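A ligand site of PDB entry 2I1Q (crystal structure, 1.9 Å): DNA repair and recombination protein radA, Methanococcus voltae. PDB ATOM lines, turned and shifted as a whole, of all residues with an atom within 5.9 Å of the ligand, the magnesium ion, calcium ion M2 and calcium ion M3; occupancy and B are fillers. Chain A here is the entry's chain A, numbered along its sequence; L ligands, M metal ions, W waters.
N of Thr 112 is in hydrogen-bond range of O6 of the ligand (2.9 Å).
The backbone NH (N) of Lys 111 sits at hydrogen-bond distance from an oxygen (O5) of the ligand, at 3.2 Å.
NZ of Lys 111 is in salt-bridge range of O5 of the ligand.
An oxygen (O6) of the ligand lies within hydrogen-bond range of the backbone NH (N) of Gln 113.
An oxygen (O7) of the ligand sits at hydrogen-bond distance from the side-chain amide nitrogen (NE2) of Gln 113 (3.5 Å).
OE1 of Gln 161 lies within hydrogen-bond range of N4 of the ligand, 3.0 Å away.
N of Gly 110 lies within hydrogen-bond range of O5 of the ligand, at 3.1 Å.
N of Ser 109 sits at hydrogen-bond distance from O5 of the ligand.
The side-chain hydroxyl of Ser 109 lies within hydrogen-bond range of an oxygen (O5) of the ligand (3.3 Å).
NZ of Lys 111 sits at hydrogen-bond distance from O of Gly 105.
OE1 of Gln 113 lies within hydrogen-bond range of NE of Arg 158 (2.8 Å).
The side-chain hydroxyl (OG) of Ser 109 sits at hydrogen-bond distance from the backbone carbonyl oxygen (O) of Val 106 (2.7 Å).
The guanidinium group of Arg 296 lies within hydrogen-bond range of the backbone carbonyl oxygen of Ser 109 (2.9 Å).
O of Glu 317 lies within hydrogen-bond range of NH2 of Arg 158, at 2.9 Å.
The backbone carbonyl oxygen (O) of Thr 316 lies within hydrogen-bond range of the guanidinium group (NH1) of Arg 158 (2.7 Å).
The backbone NH of Lys 318 lies close to the side-chain hydroxyl of Thr 316, at 3.1 Å.
O of Gly 293 sits at hydrogen-bond distance from NH1 of Arg 296, at 3.3 Å.
N1 of the ligand sits close to N of Gly 108, at 2.8 Å.
The guanidinium group (NH2) of Arg 158 sits close to a nitrogen (N4) of the ligand, at 3.4 Å.
Residues that only touch the ligand: Val 106 (3.8 Å), Phe 107 (3.7 Å), Glu 151 (3.5 Å), Arg 296 (3.9 Å), Ile 315 (3.9 Å), Thr 316 (3.4 Å) and Glu 317 (3.4 Å).
Hydrophobic or aromatic side chains within 4 Å of the ligand: Phe 107 and Ile 315.
Of the 22 residues printed, 15 come within 4 Å of the ligand.
Glu 151 touches the magnesium ion.
Two residues have an atom within 4 Å of the magnesium ion: Thr 112 and Glu 151.
No residue comes within 4 Å of calcium ion M2.
No residue comes within 4 Å of calcium ion M3.
The magnesium ion is bound by O2 of the ligand, 2.0 Å away.
The magnesium ion is bound by water W9 (2.1 Å).
The magnesium ion is bound by water W11 (2.1 Å).
OG1 of Thr 112 binds the magnesium ion (2.1 Å).
An oxygen (O4) of the ligand binds the magnesium ion, 2.1 Å away.
Water W3 binds the magnesium ion, at 2.2 Å.
Calcium ion M2 is bound by water W12 (2.3 Å), O3 of the ligand (2.5 Å), water W5 (2.5 Å) and water W1 (2.7 Å).
Calcium ion M2 has four donor atoms within binding distance.
O11 of the ligand binds calcium ion M3 (2.4 Å).
Water W10 is bound to calcium ion M3 (2.5 Å).
Water W8 binds calcium ion M3, 2.5 Å away.
Calcium ion M3 is bound by an oxygen (O12) of the ligand (2.7 Å).
Calcium ion M3 has four donor atoms within binding distance.
Water W11 lies within hydrogen-bond range of OE1 of Glu 151 (2.6 Å) and OG1 of Thr 153 (2.8 Å).
Water W8 bridges NH2 of Arg 296 (2.8 Å) and O of Gly 293 (3.4 Å).
Water W2 bridges an oxygen (O1) of the ligand (2.6 Å) and the side-chain carboxylate of Glu 151 (3.0 Å).
Water W4 bridges NE2 of Gln 161 (3.0 Å) and N5 of the ligand (3.0 Å).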
ATOM      1  N   GLY A 105     -20.689  -7.296  -9.001  1.00  0.00           N
ATOM      2  CA  GLY A 105     -22.026  -6.758  -9.141  1.00  0.00           C
ATOM      3  C   GLY A 105     -22.032  -5.341  -9.657  1.00  0.00           C
ATOM      4  O   GLY A 105     -21.020  -4.647  -9.586  1.00  0.00           O
ATOM      5  N   VAL A 106     -23.178  -4.920 -10.163  1.00  0.00           N
ATOM      6  CA  VAL A 106     -23.354  -3.578 -10.705  1.00  0.00           C
ATOM      7  C   VAL A 106     -23.112  -2.542  -9.614  1.00  0.00           C
ATOM      8  O   VAL A 106     -23.085  -2.874  -8.422  1.00  0.00           O
ATOM      9  CB  VAL A 106     -24.788  -3.404 -11.279  1.00  0.00           C
ATOM     10  CG1 VAL A 106     -25.800  -3.489 -10.149  1.00  0.00           C
ATOM     11  CG2 VAL A 106     -24.908  -2.088 -11.995  1.00  0.00           C
ATOM     12  N   PHE A 107     -22.946  -1.290 -10.022  1.00  0.00           N
ATOM     13  CA  PHE A 107     -22.718  -0.195  -9.097  1.00  0.00           C
ATOM     14  C   PHE A 107     -23.839  -0.195  -8.058  1.00  0.00           C
ATOM     15  O   PHE A 107     -24.951  -0.633  -8.337  1.00  0.00           O
ATOM     16  CB  PHE A 107     -22.745   1.133  -9.846  1.00  0.00           C
ATOM     17  CG  PHE A 107     -24.142   1.593 -10.186  1.00  0.00           C
ATOM     18  CD1 PHE A 107     -24.867   2.366  -9.278  1.00  0.00           C
ATOM     19  CD2 PHE A 107     -24.758   1.175 -11.351  1.00  0.00           C
ATOM     20  CE1 PHE A 107     -26.192   2.709  -9.528  1.00  0.00           C
ATOM     21  CE2 PHE A 107     -26.099   1.511 -11.619  1.00  0.00           C
ATOM     22  CZ  PHE A 107     -26.816   2.275 -10.703  1.00  0.00           C
ATOM     23  N   GLY A 108     -23.534   0.311  -6.862  1.00  0.00           N
ATOM     24  CA  GLY A 108     -24.535   0.398  -5.812  1.00  0.00           C
ATOM     25  C   GLY A 108     -25.142  -0.903  -5.331  1.00  0.00           C
ATOM     26  O   GLY A 108     -26.128  -0.867  -4.589  1.00  0.00           O
ATOM     27  N   SER A 109     -24.575  -2.043  -5.716  1.00  0.00           N
ATOM     28  CA  SER A 109     -25.121  -3.327  -5.294  1.00  0.00           C
ATOM     29  C   SER A 109     -24.767  -3.678  -3.844  1.00  0.00           C
ATOM     30  O   SER A 109     -25.438  -4.503  -3.210  1.00  0.00           O
ATOM     31  CB  SER A 109     -24.663  -4.447  -6.248  1.00  0.00           C
ATOM     32  OG  SER A 109     -23.251  -4.551  -6.293  1.00  0.00           O
ATOM     33  N   GLY A 110     -23.711  -3.059  -3.312  1.00  0.00           N
ATOM     34  CA  GLY A 110     -23.330  -3.321  -1.925  1.00  0.00           C
ATOM     35  C   GLY A 110     -21.999  -3.998  -1.698  1.00  0.00           C
ATOM     36  O   GLY A 110     -21.705  -4.436  -0.578  1.00  0.00           O
ATOM     37  N   LYS A 111     -21.166  -4.089  -2.725  1.00  0.00           N
ATOM     38  CA  LYS A 111     -19.864  -4.723  -2.607  1.00  0.00           C
ATOM     39  C   LYS A 111     -19.018  -4.070  -1.516  1.00  0.00           C
ATOM     40  O   LYS A 111     -18.513  -4.740  -0.611  1.00  0.00           O
ATOM     41  CB  LYS A 111     -19.110  -4.644  -3.950  1.00  0.00           C
ATOM     42  CG  LYS A 111     -19.857  -5.313  -5.097  1.00  0.00           C
ATOM     43  CD  LYS A 111     -19.044  -5.279  -6.395  1.00  0.00           C
ATOM     44  CE  LYS A 111     -18.855  -3.851  -6.903  1.00  0.00           C
ATOM     45  NZ  LYS A 111     -20.147  -3.217  -7.259  1.00  0.00           N
ATOM     46  N   THR A 112     -18.865  -2.765  -1.604  1.00  0.00           N
ATOM     47  CA  THR A 112     -18.074  -2.031  -0.619  1.00  0.00           C
ATOM     48  C   THR A 112     -18.697  -2.120   0.778  1.00  0.00           C
ATOM     49  O   THR A 112     -17.991  -2.171   1.777  1.00  0.00           O
ATOM     50  CB  THR A 112     -17.899  -0.569  -1.067  1.00  0.00           C
ATOM     51  OG1 THR A 112     -17.075  -0.545  -2.253  1.00  0.00           O
ATOM     52  CG2 THR A 112     -17.218   0.272   0.021  1.00  0.00           C
ATOM     53  N   GLN A 113     -20.027  -2.170   0.839  1.00  0.00           N
ATOM     54  CA  GLN A 113     -20.725  -2.288   2.116  1.00  0.00           C
ATOM     55  C   GLN A 113     -20.340  -3.601   2.793  1.00  0.00           C
ATOM     56  O   GLN A 113     -20.088  -3.650   4.002  1.00  0.00           O
ATOM     57  CB  GLN A 113     -22.254  -2.262   1.927  1.00  0.00           C
ATOM     58  CG  GLN A 113     -22.785  -0.961   1.330  1.00  0.00           C
ATOM     59  CD  GLN A 113     -22.335   0.267   2.103  1.00  0.00           C
ATOM     60  OE1 GLN A 113     -22.731   0.471   3.250  1.00  0.00           O
ATOM     61  NE2 GLN A 113     -21.502   1.083   1.473  1.00  0.00           N
ATOM     62  N   ILE A 114     -20.313  -4.690   2.022  1.00  0.00           N
ATOM     63  CA  ILE A 114     -19.953  -5.995   2.561  1.00  0.00           C
ATOM     64  C   ILE A 114     -18.518  -5.975   3.087  1.00  0.00           C
ATOM     65  O   ILE A 114     -18.219  -6.581   4.122  1.00  0.00           O
ATOM     66  CB  ILE A 114     -20.120  -7.109   1.490  1.00  0.00           C
ATOM     67  CG1 ILE A 114     -21.599  -7.238   1.117  1.00  0.00           C
ATOM     68  CG2 ILE A 114     -19.597  -8.443   2.024  1.00  0.00           C
ATOM     69  CD1 ILE A 114     -21.878  -8.154  -0.079  1.00  0.00           C
ATOM     70  N   GLU A 151     -10.287   2.082  -4.791  1.00  0.00           N
ATOM     71  CA  GLU A 151     -11.208   3.071  -5.349  1.00  0.00           C
ATOM     72  C   GLU A 151     -11.404   4.308  -4.489  1.00  0.00           C
ATOM     73  O   GLU A 151     -12.156   5.214  -4.864  1.00  0.00           O
ATOM     74  CB  GLU A 151     -12.554   2.423  -5.632  1.00  0.00           C
ATOM     75  CG  GLU A 151     -12.620   1.738  -6.988  1.00  0.00           C
ATOM     76  CD  GLU A 151     -13.848   0.880  -7.151  1.00  0.00           C
ATOM     77  OE1 GLU A 151     -14.940   1.313  -6.740  1.00  0.00           O
ATOM     78  OE2 GLU A 151     -13.721  -0.231  -7.720  1.00  0.00           O
ATOM     79  N   THR A 153     -12.917   4.494  -1.651  1.00  0.00           N
ATOM     80  CA  THR A 153     -14.224   4.545  -1.020  1.00  0.00           C
ATOM     81  C   THR A 153     -14.273   4.006   0.404  1.00  0.00           C
ATOM     82  O   THR A 153     -15.345   3.677   0.919  1.00  0.00           O
ATOM     83  CB  THR A 153     -15.287   3.808  -1.876  1.00  0.00           C
ATOM     84  OG1 THR A 153     -14.786   2.532  -2.276  1.00  0.00           O
ATOM     85  CG2 THR A 153     -15.626   4.631  -3.127  1.00  0.00           C
ATOM     86  N   ARG A 158     -18.744   4.991   8.023  1.00  0.00           N
ATOM     87  CA  ARG A 158     -19.554   3.804   7.839  1.00  0.00           C
ATOM     88  C   ARG A 158     -19.149   2.708   8.814  1.00  0.00           C
ATOM     89  O   ARG A 158     -19.997   1.968   9.309  1.00  0.00           O
ATOM     90  CB  ARG A 158     -19.429   3.319   6.395  1.00  0.00           C
ATOM     91  CG  ARG A 158     -20.437   2.249   6.017  1.00  0.00           C
ATOM     92  CD  ARG A 158     -21.866   2.684   6.331  1.00  0.00           C
ATOM     93  NE  ARG A 158     -22.821   1.804   5.661  1.00  0.00           N
ATOM     94  CZ  ARG A 158     -24.038   1.531   6.097  1.00  0.00           C
ATOM     95  NH1 ARG A 158     -24.821   0.713   5.391  1.00  0.00           N
ATOM     96  NH2 ARG A 158     -24.483   2.052   7.226  1.00  0.00           N
ATOM     97  N   GLN A 161     -20.673   3.648  12.186  1.00  0.00           N
ATOM     98  CA  GLN A 161     -22.110   3.429  12.174  1.00  0.00           C
ATOM     99  C   GLN A 161     -22.450   1.941  12.257  1.00  0.00           C
ATOM    100  O   GLN A 161     -23.297   1.542  13.053  1.00  0.00           O
ATOM    101  CB  GLN A 161     -22.719   4.058  10.921  1.00  0.00           C
ATOM    102  CG  GLN A 161     -24.224   3.872  10.787  1.00  0.00           C
ATOM    103  CD  GLN A 161     -24.802   4.627   9.615  1.00  0.00           C
ATOM    104  OE1 GLN A 161     -24.274   4.557   8.495  1.00  0.00           O
ATOM    105  NE2 GLN A 161     -25.884   5.355   9.850  1.00  0.00           N
ATOM    106  N   ASP A 211     -10.706  -4.027  -2.476  1.00  0.00           N
ATOM    107  CA  ASP A 211     -11.841  -3.339  -3.094  1.00  0.00           C
ATOM    108  C   ASP A 211     -11.292  -2.129  -3.838  1.00  0.00           C
ATOM    109  O   ASP A 211     -10.936  -1.129  -3.199  1.00  0.00           O
ATOM    110  CB  ASP A 211     -12.818  -2.905  -1.986  1.00  0.00           C
ATOM    111  CG  ASP A 211     -14.039  -2.174  -2.518  1.00  0.00           C
ATOM    112  OD1 ASP A 211     -14.470  -2.464  -3.650  1.00  0.00           O
ATOM    113  OD2 ASP A 211     -14.574  -1.332  -1.778  1.00  0.00           O
ATOM    114  N   GLN A 257     -15.999  -5.548 -10.545  1.00  0.00           N
ATOM    115  CA  GLN A 257     -16.995  -4.808 -11.302  1.00  0.00           C
ATOM    116  C   GLN A 257     -17.548  -5.730 -12.384  1.00  0.00           C
ATOM    117  O   GLN A 257     -17.048  -6.847 -12.564  1.00  0.00           O
ATOM    118  CB  GLN A 257     -16.371  -3.549 -11.916  1.00  0.00           C
ATOM    119  CG  GLN A 257     -15.699  -2.652 -10.870  1.00  0.00           C
ATOM    120  CD  GLN A 257     -15.078  -1.402 -11.467  1.00  0.00           C
ATOM    121  OE1 GLN A 257     -14.704  -1.371 -12.645  1.00  0.00           O
ATOM    122  NE2 GLN A 257     -14.946  -0.356 -10.654  1.00  0.00           N
ATOM    123  N   GLY A 293     -35.870  -1.216  -3.376  1.00  0.00           N
ATOM    124  CA  GLY A 293     -35.341  -0.416  -2.283  1.00  0.00           C
ATOM    125  C   GLY A 293     -33.989  -0.871  -1.767  1.00  0.00           C
ATOM    126  O   GLY A 293     -33.000  -0.880  -2.493  1.00  0.00           O
ATOM    127  N   ARG A 296     -31.450  -6.760  -1.486  1.00  0.00           N
ATOM    128  CA  ARG A 296     -30.364  -7.227  -2.338  1.00  0.00           C
ATOM    129  C   ARG A 296     -30.425  -8.737  -2.452  1.00  0.00           C
ATOM    130  O   ARG A 296     -30.989  -9.408  -1.594  1.00  0.00           O
ATOM    131  CB  ARG A 296     -29.007  -6.819  -1.754  1.00  0.00           C
ATOM    132  CG  ARG A 296     -28.790  -5.310  -1.622  1.00  0.00           C
ATOM    133  CD  ARG A 296     -28.538  -4.678  -2.971  1.00  0.00           C
ATOM    134  NE  ARG A 296     -28.063  -3.303  -2.836  1.00  0.00           N
ATOM    135  CZ  ARG A 296     -28.840  -2.274  -2.491  1.00  0.00           C
ATOM    136  NH1 ARG A 296     -30.135  -2.456  -2.263  1.00  0.00           N
ATOM    137  NH2 ARG A 296     -28.309  -1.060  -2.370  1.00  0.00           N
ATOM    138  N   ILE A 315     -29.487  -3.714   2.872  1.00  0.00           N
ATOM    139  CA  ILE A 315     -28.423  -2.805   3.235  1.00  0.00           C
ATOM    140  C   ILE A 315     -29.128  -1.582   3.831  1.00  0.00           C
ATOM    141  O   ILE A 315     -29.849  -0.876   3.131  1.00  0.00           O
ATOM    142  CB  ILE A 315     -27.572  -2.376   2.034  1.00  0.00           C
ATOM    143  CG1 ILE A 315     -26.920  -3.612   1.399  1.00  0.00           C
ATOM    144  CG2 ILE A 315     -26.509  -1.384   2.473  1.00  0.00           C
ATOM    145  CD1 ILE A 315     -26.031  -3.291   0.217  1.00  0.00           C
ATOM    146  N   THR A 316     -28.916  -1.352   5.118  1.00  0.00           N
ATOM    147  CA  THR A 316     -29.571  -0.247   5.822  1.00  0.00           C
ATOM    148  C   THR A 316     -28.529   0.574   6.580  1.00  0.00           C
ATOM    149  O   THR A 316     -27.330   0.336   6.449  1.00  0.00           O
ATOM    150  CB  THR A 316     -30.584  -0.784   6.834  1.00  0.00           C
ATOM    151  OG1 THR A 316     -29.869  -1.471   7.885  1.00  0.00           O
ATOM    152  CG2 THR A 316     -31.543  -1.766   6.169  1.00  0.00           C
ATOM    153  N   GLU A 317     -28.984   1.530   7.382  1.00  0.00           N
ATOM    154  CA  GLU A 317     -28.037   2.335   8.160  1.00  0.00           C
ATOM    155  C   GLU A 317     -27.267   1.427   9.108  1.00  0.00           C
ATOM    156  O   GLU A 317     -26.186   1.779   9.575  1.00  0.00           O
ATOM    157  CB  GLU A 317     -28.754   3.441   8.955  1.00  0.00           C
ATOM    158  CG  GLU A 317     -30.265   3.392   8.937  1.00  0.00           C
ATOM    159  CD  GLU A 317     -30.838   2.204   9.665  1.00  0.00           C
ATOM    160  OE1 GLU A 317     -30.497   2.018  10.855  1.00  0.00           O
ATOM    161  OE2 GLU A 317     -31.625   1.459   9.052  1.00  0.00           O
ATOM    162  N   LYS A 318     -27.832   0.257   9.402  1.00  0.00           N
ATOM    163  CA  LYS A 318     -27.176  -0.678  10.302  1.00  0.00           C
ATOM    164  C   LYS A 318     -26.133  -1.528   9.587  1.00  0.00           C
ATOM    165  O   LYS A 318     -25.346  -2.228  10.223  1.00  0.00           O
ATOM    166  CB  LYS A 318     -28.209  -1.589  10.959  1.00  0.00           C
ATOM    167  CG  LYS A 318     -29.238  -0.840  11.785  1.00  0.00           C
ATOM    168  CD  LYS A 318     -30.177  -1.793  12.495  1.00  0.00           C
ATOM    169  CE  LYS A 318     -31.147  -1.020  13.379  1.00  0.00           C
ATOM    170  NZ  LYS A 318     -32.056  -1.939  14.135  1.00  0.00           N
HETATM  171  P1  LIG L   1     -19.459   0.631  -6.748  1.00  0.00           P
HETATM  172  O1  LIG L   1     -19.078  -0.535  -7.479  1.00  0.00           O
HETATM  173  O2  LIG L   1     -18.332   1.033  -5.858  1.00  0.00           O
HETATM  174  O3  LIG L   1     -19.777   1.613  -7.776  1.00  0.00           O
HETATM  175  P2  LIG L   1     -20.930  -0.730  -4.673  1.00  0.00           P
HETATM  176  O4  LIG L   1     -19.587  -1.000  -4.098  1.00  0.00           O
HETATM  177  O5  LIG L   1     -21.414  -2.019  -5.131  1.00  0.00           O
HETATM  178  N1  LIG L   1     -20.857   0.193  -5.952  1.00  0.00           N
HETATM  179  P3  LIG L   1     -21.813   0.133  -2.107  1.00  0.00           P
HETATM  180  O6  LIG L   1     -21.210  -1.097  -1.414  1.00  0.00           O
HETATM  181  O7  LIG L   1     -20.952   1.317  -1.961  1.00  0.00           O
HETATM  182  O8  LIG L   1     -22.041  -0.148  -3.675  1.00  0.00           O
HETATM  183  O9  LIG L   1     -23.298   0.412  -1.451  1.00  0.00           O
HETATM  184  C1  LIG L   1     -24.152   1.560  -1.949  1.00  0.00           C
HETATM  185  C2  LIG L   1     -25.360   1.477  -1.391  1.00  0.00           C
HETATM  186  O10 LIG L   1     -25.179   1.393   0.060  1.00  0.00           O
HETATM  187  C3  LIG L   1     -26.073   2.839  -1.581  1.00  0.00           C
HETATM  188  O11 LIG L   1     -26.455   3.138  -2.881  1.00  0.00           O
HETATM  189  C4  LIG L   1     -26.947   3.029  -0.306  1.00  0.00           C
HETATM  190  O12 LIG L   1     -28.323   2.462  -0.656  1.00  0.00           O
HETATM  191  C5  LIG L   1     -26.277   2.087   0.719  1.00  0.00           C
HETATM  192  N2  LIG L   1     -25.753   2.813   1.751  1.00  0.00           N
HETATM  193  C6  LIG L   1     -24.459   3.355   1.833  1.00  0.00           C
HETATM  194  N3  LIG L   1     -24.313   3.976   2.955  1.00  0.00           N
HETATM  195  C7  LIG L   1     -25.474   3.884   3.654  1.00  0.00           C
HETATM  196  C8  LIG L   1     -25.882   4.353   4.900  1.00  0.00           C
HETATM  197  N4  LIG L   1     -25.037   5.084   5.677  1.00  0.00           N
HETATM  198  N5  LIG L   1     -27.190   4.075   5.339  1.00  0.00           N
HETATM  199  C9  LIG L   1     -28.086   3.310   4.535  1.00  0.00           C
HETATM  200  N6  LIG L   1     -27.712   2.837   3.303  1.00  0.00           N
HETATM  201  C10 LIG L   1     -26.383   3.153   2.911  1.00  0.00           C
HETATM  202 MG    MG M   1     -17.763   0.133  -4.169  1.00  0.00          MG
HETATM  203 CA    CA M   2     -19.435   4.084  -7.879  1.00  0.00          CA
HETATM  204 CA    CA M   3     -28.877   3.053  -3.230  1.00  0.00          CA
HETATM  205  O   HOH W   1     -19.850   4.813  -5.338  1.00  0.00           O
HETATM  206  O   HOH W   2     -16.561  -1.170  -7.641  1.00  0.00           O
HETATM  207  O   HOH W   3     -16.635  -1.611  -4.871  1.00  0.00           O
HETATM  208  O   HOH W   4     -27.548   6.081   7.520  1.00  0.00           O
HETATM  209  O   HOH W   5     -17.509   3.375  -6.402  1.00  0.00           O
HETATM  210  O   HOH W   6     -30.002   0.614   0.423  1.00  0.00           O
HETATM  211  O   HOH W   7     -29.792   3.675   1.304  1.00  0.00           O
HETATM  212  O   HOH W   8     -30.216   1.015  -2.606  1.00  0.00           O
HETATM  213  O   HOH W   9     -18.667   1.761  -3.256  1.00  0.00           O
HETATM  214  O   HOH W  10     -27.895   1.410  -4.854  1.00  0.00           O
HETATM  215  O   HOH W  11     -15.992   1.194  -4.391  1.00  0.00           O
HETATM  216  O   HOH W  12     -21.670   4.594  -7.749  1.00  0.00           O
